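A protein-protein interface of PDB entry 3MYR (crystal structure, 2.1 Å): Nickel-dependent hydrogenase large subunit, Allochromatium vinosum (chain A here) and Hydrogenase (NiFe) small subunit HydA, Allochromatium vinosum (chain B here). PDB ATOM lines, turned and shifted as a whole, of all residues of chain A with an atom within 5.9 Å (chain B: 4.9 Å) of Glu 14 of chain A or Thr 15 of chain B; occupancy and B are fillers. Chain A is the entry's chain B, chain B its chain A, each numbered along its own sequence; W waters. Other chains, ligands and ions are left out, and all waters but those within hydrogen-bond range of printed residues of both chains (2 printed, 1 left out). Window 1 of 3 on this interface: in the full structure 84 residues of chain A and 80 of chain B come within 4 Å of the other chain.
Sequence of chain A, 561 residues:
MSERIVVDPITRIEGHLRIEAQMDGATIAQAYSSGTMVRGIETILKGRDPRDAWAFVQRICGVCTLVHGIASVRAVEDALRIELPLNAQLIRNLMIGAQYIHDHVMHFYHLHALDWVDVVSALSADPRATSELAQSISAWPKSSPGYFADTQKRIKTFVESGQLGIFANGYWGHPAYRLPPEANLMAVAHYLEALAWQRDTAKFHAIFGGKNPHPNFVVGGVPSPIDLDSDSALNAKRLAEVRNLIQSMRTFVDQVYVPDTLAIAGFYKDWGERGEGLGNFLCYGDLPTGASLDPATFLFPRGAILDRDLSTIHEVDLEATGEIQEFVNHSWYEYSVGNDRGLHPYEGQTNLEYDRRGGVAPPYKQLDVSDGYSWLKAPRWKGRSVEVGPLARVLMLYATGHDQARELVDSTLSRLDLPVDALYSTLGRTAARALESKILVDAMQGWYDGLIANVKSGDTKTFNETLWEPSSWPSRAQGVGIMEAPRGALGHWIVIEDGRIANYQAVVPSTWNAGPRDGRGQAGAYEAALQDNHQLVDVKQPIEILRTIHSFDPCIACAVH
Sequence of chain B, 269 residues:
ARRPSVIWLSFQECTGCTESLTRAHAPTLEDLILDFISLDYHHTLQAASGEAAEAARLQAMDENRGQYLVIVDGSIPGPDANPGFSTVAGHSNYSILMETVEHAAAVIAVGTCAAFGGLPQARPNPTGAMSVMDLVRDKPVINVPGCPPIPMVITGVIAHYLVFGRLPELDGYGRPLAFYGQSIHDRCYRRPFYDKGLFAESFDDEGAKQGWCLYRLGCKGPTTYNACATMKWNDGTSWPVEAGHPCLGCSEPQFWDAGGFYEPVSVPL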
ATOM      1  N   ARG A  12      -1.493 -12.986 -19.048  1.00  0.00           N
ATOM      2  CA  ARG A  12      -0.898 -14.284 -19.312  1.00  0.00           C
ATOM      3  C   ARG A  12      -0.026 -14.739 -18.172  1.00  0.00           C
ATOM      4  O   ARG A  12       1.047 -15.317 -18.385  1.00  0.00           O
ATOM      5  CB  ARG A  12      -0.179 -14.294 -20.669  1.00  0.00           C
ATOM      6  CG  ARG A  12      -1.252 -14.513 -21.758  1.00  0.00           C
ATOM      7  CD  ARG A  12      -0.653 -14.539 -23.168  1.00  0.00           C
ATOM      8  NE  ARG A  12       0.004 -13.270 -23.523  1.00  0.00           N
ATOM      9  CZ  ARG A  12       1.311 -13.102 -23.761  1.00  0.00           C
ATOM     10  NH1 ARG A  12       2.204 -14.095 -23.657  1.00  0.00           N
ATOM     11  NH2 ARG A  12       1.752 -11.919 -24.192  1.00  0.00           N
ATOM     12  N   ILE A  13      -0.470 -14.412 -16.956  1.00  0.00           N
ATOM     13  CA  ILE A  13      -0.027 -15.114 -15.765  1.00  0.00           C
ATOM     14  C   ILE A  13      -1.288 -15.515 -15.011  1.00  0.00           C
ATOM     15  O   ILE A  13      -2.428 -15.210 -15.434  1.00  0.00           O
ATOM     16  CB  ILE A  13       0.844 -14.160 -14.838  1.00  0.00           C
ATOM     17  CG1 ILE A  13       0.006 -12.939 -14.366  1.00  0.00           C
ATOM     18  CG2 ILE A  13       2.015 -13.648 -15.581  1.00  0.00           C
ATOM     19  CD1 ILE A  13       0.633 -12.159 -13.182  1.00  0.00           C
ATOM     20  N   GLU A  14      -1.092 -16.136 -13.858  1.00  0.00           N
ATOM     21  CA  GLU A  14      -2.190 -16.247 -12.890  1.00  0.00           C
ATOM     22  C   GLU A  14      -2.113 -15.069 -11.904  1.00  0.00           C
ATOM     23  O   GLU A  14      -1.049 -14.761 -11.382  1.00  0.00           O
ATOM     24  CB  GLU A  14      -2.058 -17.559 -12.107  1.00  0.00           C
ATOM     25  CG  GLU A  14      -3.356 -17.877 -11.262  1.00  0.00           C
ATOM     26  CD  GLU A  14      -3.644 -16.822 -10.162  1.00  0.00           C
ATOM     27  OE1 GLU A  14      -4.880 -16.507  -9.938  1.00  0.00           O
ATOM     28  OE2 GLU A  14      -2.655 -16.310  -9.542  1.00  0.00           O
ATOM     29  N   GLY A  15      -3.214 -14.375 -11.705  1.00  0.00           N
ATOM     30  CA  GLY A  15      -3.296 -13.392 -10.659  1.00  0.00           C
ATOM     31  C   GLY A  15      -2.815 -12.014 -11.028  1.00  0.00           C
ATOM     32  O   GLY A  15      -2.716 -11.662 -12.200  1.00  0.00           O
ATOM     33  N   HIS A  16      -2.495 -11.219 -10.007  1.00  0.00           N
ATOM     34  CA  HIS A  16      -2.480  -9.766 -10.160  1.00  0.00           C
ATOM     35  C   HIS A  16      -1.105  -9.186  -9.905  1.00  0.00           C
ATOM     36  O   HIS A  16      -0.717  -9.024  -8.750  1.00  0.00           O
ATOM     37  CB  HIS A  16      -3.519  -9.141  -9.199  1.00  0.00           C
ATOM     38  CG  HIS A  16      -4.920  -9.416  -9.634  1.00  0.00           C
ATOM     39  ND1 HIS A  16      -5.742 -10.334  -8.999  1.00  0.00           N
ATOM     40  CD2 HIS A  16      -5.580  -9.033 -10.747  1.00  0.00           C
ATOM     41  CE1 HIS A  16      -6.906 -10.393  -9.630  1.00  0.00           C
ATOM     42  NE2 HIS A  16      -6.815  -9.639 -10.713  1.00  0.00           N
ATOM     43  N   ILE A  60      -6.019 -21.649  -2.549  1.00  0.00           N
ATOM     44  CA  ILE A  60      -5.008 -20.639  -2.861  1.00  0.00           C
ATOM     45  C   ILE A  60      -4.910 -20.456  -4.370  1.00  0.00           C
ATOM     46  O   ILE A  60      -4.729 -19.338  -4.869  1.00  0.00           O
ATOM     47  CB  ILE A  60      -3.627 -21.026  -2.239  1.00  0.00           C
ATOM     48  CG1 ILE A  60      -3.749 -20.739  -0.722  1.00  0.00           C
ATOM     49  CG2 ILE A  60      -2.464 -20.203  -2.920  1.00  0.00           C
ATOM     50  CD1 ILE A  60      -2.457 -21.286   0.108  1.00  0.00           C
ATOM     51  N   CYS A  61      -5.005 -21.552  -5.126  1.00  0.00           N
ATOM     52  CA  CYS A  61      -4.753 -21.402  -6.554  1.00  0.00           C
ATOM     53  C   CYS A  61      -5.270 -22.558  -7.353  1.00  0.00           C
ATOM     54  O   CYS A  61      -5.043 -23.690  -6.999  1.00  0.00           O
ATOM     55  CB  CYS A  61      -3.267 -21.171  -6.855  1.00  0.00           C
ATOM     56  SG  CYS A  61      -3.042 -20.693  -8.611  1.00  0.00           S
ATOM     57  N   GLY A  62      -6.015 -22.259  -8.408  1.00  0.00           N
ATOM     58  CA  GLY A  62      -6.553 -23.304  -9.237  1.00  0.00           C
ATOM     59  C   GLY A  62      -5.765 -23.575 -10.512  1.00  0.00           C
ATOM     60  O   GLY A  62      -6.164 -24.427 -11.329  1.00  0.00           O
ATOM     61  N   VAL A  63      -4.652 -22.869 -10.728  1.00  0.00           N
ATOM     62  CA  VAL A  63      -3.777 -23.197 -11.881  1.00  0.00           C
ATOM     63  C   VAL A  63      -2.826 -24.289 -11.402  1.00  0.00           C
ATOM     64  O   VAL A  63      -2.811 -25.375 -11.972  1.00  0.00           O
ATOM     65  CB  VAL A  63      -2.943 -21.989 -12.359  1.00  0.00           C
ATOM     66  CG1 VAL A  63      -1.939 -22.448 -13.477  1.00  0.00           C
ATOM     67  CG2 VAL A  63      -3.877 -20.992 -12.916  1.00  0.00           C
ATOM     68  N   LEU A 111       0.155 -19.342 -22.104  1.00  0.00           N
ATOM     69  CA  LEU A 111       0.669 -18.160 -21.364  1.00  0.00           C
ATOM     70  C   LEU A 111       1.964 -17.564 -21.941  1.00  0.00           C
ATOM     71  O   LEU A 111       2.065 -16.347 -22.062  1.00  0.00           O
ATOM     72  CB  LEU A 111       0.849 -18.432 -19.856  1.00  0.00           C
ATOM     73  CG  LEU A 111      -0.403 -19.077 -19.171  1.00  0.00           C
ATOM     74  CD1 LEU A 111      -0.193 -19.123 -17.631  1.00  0.00           C
ATOM     75  CD2 LEU A 111      -1.648 -18.394 -19.406  1.00  0.00           C
ATOM     76  N   PRO A 213     -10.680 -28.650 -12.119  1.00  0.00           N
ATOM     77  CA  PRO A 213      -9.755 -28.341 -10.999  1.00  0.00           C
ATOM     78  C   PRO A 213     -10.219 -28.784  -9.579  1.00  0.00           C
ATOM     79  O   PRO A 213     -11.406 -29.085  -9.344  1.00  0.00           O
ATOM     80  CB  PRO A 213      -9.634 -26.791 -11.049  1.00  0.00           C
ATOM     81  CG  PRO A 213     -10.060 -26.406 -12.556  1.00  0.00           C
ATOM     82  CD  PRO A 213     -11.187 -27.408 -12.753  1.00  0.00           C
ATOM     83  N   PRO A 554       4.690 -16.855 -13.356  1.00  0.00           N
ATOM     84  CA  PRO A 554       4.196 -16.256 -12.093  1.00  0.00           C
ATOM     85  C   PRO A 554       2.774 -16.689 -11.725  1.00  0.00           C
ATOM     86  O   PRO A 554       1.922 -16.858 -12.593  1.00  0.00           O
ATOM     87  CB  PRO A 554       4.179 -14.746 -12.374  1.00  0.00           C
ATOM     88  CG  PRO A 554       5.103 -14.542 -13.588  1.00  0.00           C
ATOM     89  CD  PRO A 554       5.038 -15.834 -14.362  1.00  0.00           C
ATOM     90  N   CYS A 555       2.516 -16.817 -10.431  1.00  0.00           N
ATOM     91  CA  CYS A 555       1.182 -17.061  -9.938  1.00  0.00           C
ATOM     92  C   CYS A 555       1.033 -16.251  -8.652  1.00  0.00           C
ATOM     93  O   CYS A 555       1.677 -16.552  -7.644  1.00  0.00           O
ATOM     94  CB  CYS A 555       0.990 -18.561  -9.682  1.00  0.00           C
ATOM     95  SG  CYS A 555      -0.715 -18.819  -9.034  1.00  0.00           S
ATOM     96  N   ILE A 556       0.235 -15.180  -8.695  1.00  0.00           N
ATOM     97  CA  ILE A 556       0.225 -14.200  -7.574  1.00  0.00           C
ATOM     98  C   ILE A 556      -0.825 -14.640  -6.559  1.00  0.00           C
ATOM     99  O   ILE A 556      -0.769 -14.273  -5.381  1.00  0.00           O
ATOM    100  CB  ILE A 556      -0.032 -12.750  -8.063  1.00  0.00           C
ATOM    101  CG1 ILE A 556       1.095 -12.274  -9.064  1.00  0.00           C
ATOM    102  CG2 ILE A 556      -0.081 -11.807  -6.895  1.00  0.00           C
ATOM    103  CD1 ILE A 556       2.544 -12.743  -8.799  1.00  0.00           C
ATOM    104  N   ALA A 557      -1.791 -15.434  -7.000  1.00  0.00           N
ATOM    105  CA  ALA A 557      -2.715 -15.980  -5.992  1.00  0.00           C
ATOM    106  C   ALA A 557      -1.877 -16.936  -5.124  1.00  0.00           C
ATOM    107  O   ALA A 557      -1.919 -16.857  -3.886  1.00  0.00           O
ATOM    108  CB  ALA A 557      -3.897 -16.780  -6.693  1.00  0.00           C
ATOM    109  N   CYS A 558      -1.043 -17.784  -5.740  1.00  0.00           N
ATOM    110  CA  CYS A 558      -0.120 -18.558  -4.902  1.00  0.00           C
ATOM    111  C   CYS A 558       0.797 -17.675  -4.061  1.00  0.00           C
ATOM    112  O   CYS A 558       1.025 -17.947  -2.878  1.00  0.00           O
ATOM    113  CB  CYS A 558       0.794 -19.394  -5.784  1.00  0.00           C
ATOM    114  SG  CYS A 558       0.124 -20.994  -6.134  1.00  0.00           S
ATOM    115  N   GLU B  13      -9.818 -14.096  -7.007  1.00  0.00           N
ATOM    116  CA  GLU B  13     -10.085 -15.461  -7.442  1.00  0.00           C
ATOM    117  C   GLU B  13      -8.802 -16.303  -7.305  1.00  0.00           C
ATOM    118  O   GLU B  13      -7.662 -15.747  -7.153  1.00  0.00           O
ATOM    119  CB  GLU B  13     -10.583 -15.543  -8.882  1.00  0.00           C
ATOM    120  CG  GLU B  13     -10.111 -14.472  -9.812  1.00  0.00           C
ATOM    121  CD  GLU B  13      -8.788 -14.723 -10.558  1.00  0.00           C
ATOM    122  OE1 GLU B  13      -7.804 -13.900 -10.387  1.00  0.00           O
ATOM    123  OE2 GLU B  13      -8.806 -15.575 -11.478  1.00  0.00           O
ATOM    124  N   CYS B  14      -8.956 -17.614  -7.506  1.00  0.00           N
ATOM    125  CA  CYS B  14      -7.767 -18.456  -7.462  1.00  0.00           C
ATOM    126  C   CYS B  14      -7.462 -18.943  -8.899  1.00  0.00           C
ATOM    127  O   CYS B  14      -6.491 -19.659  -9.122  1.00  0.00           O
ATOM    128  CB  CYS B  14      -8.075 -19.636  -6.479  1.00  0.00           C
ATOM    129  SG  CYS B  14      -9.052 -21.016  -7.264  1.00  0.00           S
ATOM    130  N   THR B  15      -8.343 -18.571  -9.851  1.00  0.00           N
ATOM    131  CA  THR B  15      -8.248 -18.872 -11.293  1.00  0.00           C
ATOM    132  C   THR B  15      -8.771 -20.301 -11.602  1.00  0.00           C
ATOM    133  O   THR B  15      -8.874 -20.698 -12.755  1.00  0.00           O
ATOM    134  CB  THR B  15      -6.842 -18.516 -11.945  1.00  0.00           C
ATOM    135  OG1 THR B  15      -6.461 -17.155 -11.595  1.00  0.00           O
ATOM    136  CG2 THR B  15      -6.864 -18.625 -13.544  1.00  0.00           C
ATOM    137  N   GLY B  16      -9.191 -21.029 -10.575  1.00  0.00           N
ATOM    138  CA  GLY B  16      -9.963 -22.268 -10.777  1.00  0.00           C
ATOM    139  C   GLY B  16     -11.144 -22.165 -11.719  1.00  0.00           C
ATOM    140  O   GLY B  16     -11.415 -23.123 -12.500  1.00  0.00           O
ATOM    141  N   CYS B  17     -11.851 -21.031 -11.693  1.00  0.00           N
ATOM    142  CA  CYS B  17     -13.037 -20.939 -12.522  1.00  0.00           C
ATOM    143  C   CYS B  17     -12.666 -20.800 -13.979  1.00  0.00           C
ATOM    144  O   CYS B  17     -13.343 -21.346 -14.856  1.00  0.00           O
ATOM    145  CB  CYS B  17     -13.993 -19.791 -12.026  1.00  0.00           C
ATOM    146  SG  CYS B  17     -14.620 -20.124 -10.331  1.00  0.00           S
ATOM    147  N   THR B  18     -11.604 -20.035 -14.280  1.00  0.00           N
ATOM    148  CA  THR B  18     -11.144 -19.986 -15.661  1.00  0.00           C
ATOM    149  C   THR B  18     -10.592 -21.344 -16.132  1.00  0.00           C
ATOM    150  O   THR B  18     -10.862 -21.777 -17.247  1.00  0.00           O
ATOM    151  CB  THR B  18     -10.015 -18.853 -15.811  1.00  0.00           C
ATOM    152  OG1 THR B  18     -10.711 -17.601 -15.811  1.00  0.00           O
ATOM    153  CG2 THR B  18      -9.222 -19.053 -17.136  1.00  0.00           C
ATOM    154  N   GLU B  19      -9.854 -22.044 -15.249  1.00  0.00           N
ATOM    155  CA  GLU B  19      -9.317 -23.343 -15.648  1.00  0.00           C
ATOM    156  C   GLU B  19     -10.497 -24.225 -15.955  1.00  0.00           C
ATOM    157  O   GLU B  19     -10.452 -24.974 -16.901  1.00  0.00           O
ATOM    158  CB  GLU B  19      -8.446 -24.013 -14.558  1.00  0.00           C
ATOM    159  CG  GLU B  19      -7.132 -23.257 -14.407  1.00  0.00           C
ATOM    160  CD  GLU B  19      -6.071 -23.655 -15.444  1.00  0.00           C
ATOM    161  OE1 GLU B  19      -4.986 -23.050 -15.369  1.00  0.00           O
ATOM    162  OE2 GLU B  19      -6.224 -24.594 -16.271  1.00  0.00           O
ATOM    163  N   THR B  44      -6.033 -13.928 -18.126  1.00  0.00           N
ATOM    164  CA  THR B  44      -5.254 -15.158 -18.246  1.00  0.00           C
ATOM    165  C   THR B  44      -4.711 -15.357 -19.652  1.00  0.00           C
ATOM    166  O   THR B  44      -3.664 -15.986 -19.831  1.00  0.00           O
ATOM    167  CB  THR B  44      -6.062 -16.406 -17.791  1.00  0.00           C
ATOM    168  OG1 THR B  44      -6.561 -16.165 -16.477  1.00  0.00           O
ATOM    169  CG2 THR B  44      -5.160 -17.655 -17.738  1.00  0.00           C
ATOM    170  N   ASP B  73     -15.237 -13.477 -11.846  1.00  0.00           N
ATOM    171  CA  ASP B  73     -14.593 -14.567 -11.150  1.00  0.00           C
ATOM    172  C   ASP B  73     -14.021 -13.919  -9.852  1.00  0.00           C
ATOM    173  O   ASP B  73     -13.260 -12.951  -9.951  1.00  0.00           O
ATOM    174  CB  ASP B  73     -13.393 -15.029 -12.035  1.00  0.00           C
ATOM    175  CG  ASP B  73     -12.888 -16.320 -11.598  1.00  0.00           C
ATOM    176  OD1 ASP B  73     -13.469 -16.770 -10.592  1.00  0.00           O
ATOM    177  OD2 ASP B  73     -11.917 -16.876 -12.145  1.00  0.00           O
HETATM  178  O   HOH W   1      -5.655 -14.747 -12.863  1.00  0.00           O
HETATM  179  O   HOH W   2      -5.676 -14.149  -8.481  1.00  0.00           O
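The backbone NH (N) of Gly 62 of chain A lies within hydrogen-bond range of the backbone carbonyl oxygen (O) of Cys 14 of chain B, 2.7 Å away. OE1 of Glu 14 of chain A sits close to OG1 of Thr 15 of chain B (2.4 Å). The backbone carbonyl oxygen of Cys 14 of chain B sits close to the side-chain sulfur of Cys 61 of chain A, 3.6 Å away.
The side-chain sulfur (SG) of Cys 14 of chain B sits close to the backbone NH (N) of Gly 16 of chain B, 3.3 Å away. O of Leu 111 of chain A sits at hydrogen-bond distance from NH1 of Arg 12 of chain A (2.8 Å). The side-chain carboxylate (OE2) of Glu 14 of chain A is in hydrogen-bond range of the backbone NH (N) of Ala 557 of chain A, 2.8 Å away. The backbone carbonyl oxygen of Glu 14 of chain A sits at hydrogen-bond distance from the backbone NH of Ile 556 of chain A, 3.0 Å away. The side-chain carboxylate (OE2) of Glu 14 of chain A lies close to the side-chain sulfur (SG) of Cys 555 of chain A (3.2 Å). SG of Cys 61 of chain A lies close to N of Val 63 of chain A (3.4 Å).
Among the printed residues, merely in contact across the chains: Leu 111 of chain A with Thr 44 of chain B, Arg 12 of chain A with Thr 44 of chain B, Val 63 of chain A with Glu 19 of chain B, Gly 62 of chain A with Glu 19 of chain B, Pro 213 of chain A with Glu 19 of chain B, Pro 213 of chain A with Gly 16 of chain B, Glu 14 of chain A with Cys 14 of chain B, His 16 of chain A with Glu 13 of chain B, Ile 60 of chain A with Cys 14 of chain B, Gly 62 of chain A with Gly 16 of chain B, Val 63 of chain A with Thr 15 of chain B, Ala 557 of chain A with Glu 13 of chain B, Glu 14 of chain A with Glu 13 of chain B and Ile 13 of chain A with Thr 44 of chain B.
Of chain B, only Glu 13 (3.9 Å), Cys 14 (3.6 Å) and Thr 15 (2.4 Å) come within 4 Å of Glu 14 of chain A. Printed residues of chain B within 4 Å of Cys 61 of chain A: Cys 14. Printed residues of chain B within 4 Å of Leu 111 of chain A: Thr 44 (3.2 Å). Printed residues of chain A within 4 Å of Glu 13 of chain B: Glu 14, His 16 and Ala 557. Printed residues of chain A within 4 Å of Cys 14 of chain B: Glu 14 (3.6 Å), Ile 60 (3.7 Å), Cys 61 (3.6 Å) and Gly 62 (2.7 Å). Thr 15 of chain B touches just these residues of chain A: Glu 14 and Val 63. Cys 17 of chain B touches none of the printed residues of chain A. Asp 73 of chain B touches none of the printed residues of chain A. The nearest residue of chain A that does not touch Thr 15 of chain B is Gly 15 of chain A (4.3 Å). The nearest printed residue of chain B that does not touch Gly 62 of chain A is Thr 15 of chain B (4.4 Å).
Of the 9 printed residues of chain B, 6 touch a printed residue of chain A. Printed residues of chain B that touch a printed residue of chain A: Glu 13, Cys 14, Thr 15, Gly 16, Glu 19 and Thr 44. Of the 16 printed residues of chain A, 11 touch a printed residue of chain B. Among the printed residues, 17 pairs touch across the chains.
Water W2 lies within hydrogen-bond range of OE1 of Glu 13 of chain B and OE1 of Glu 14 of chain A.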
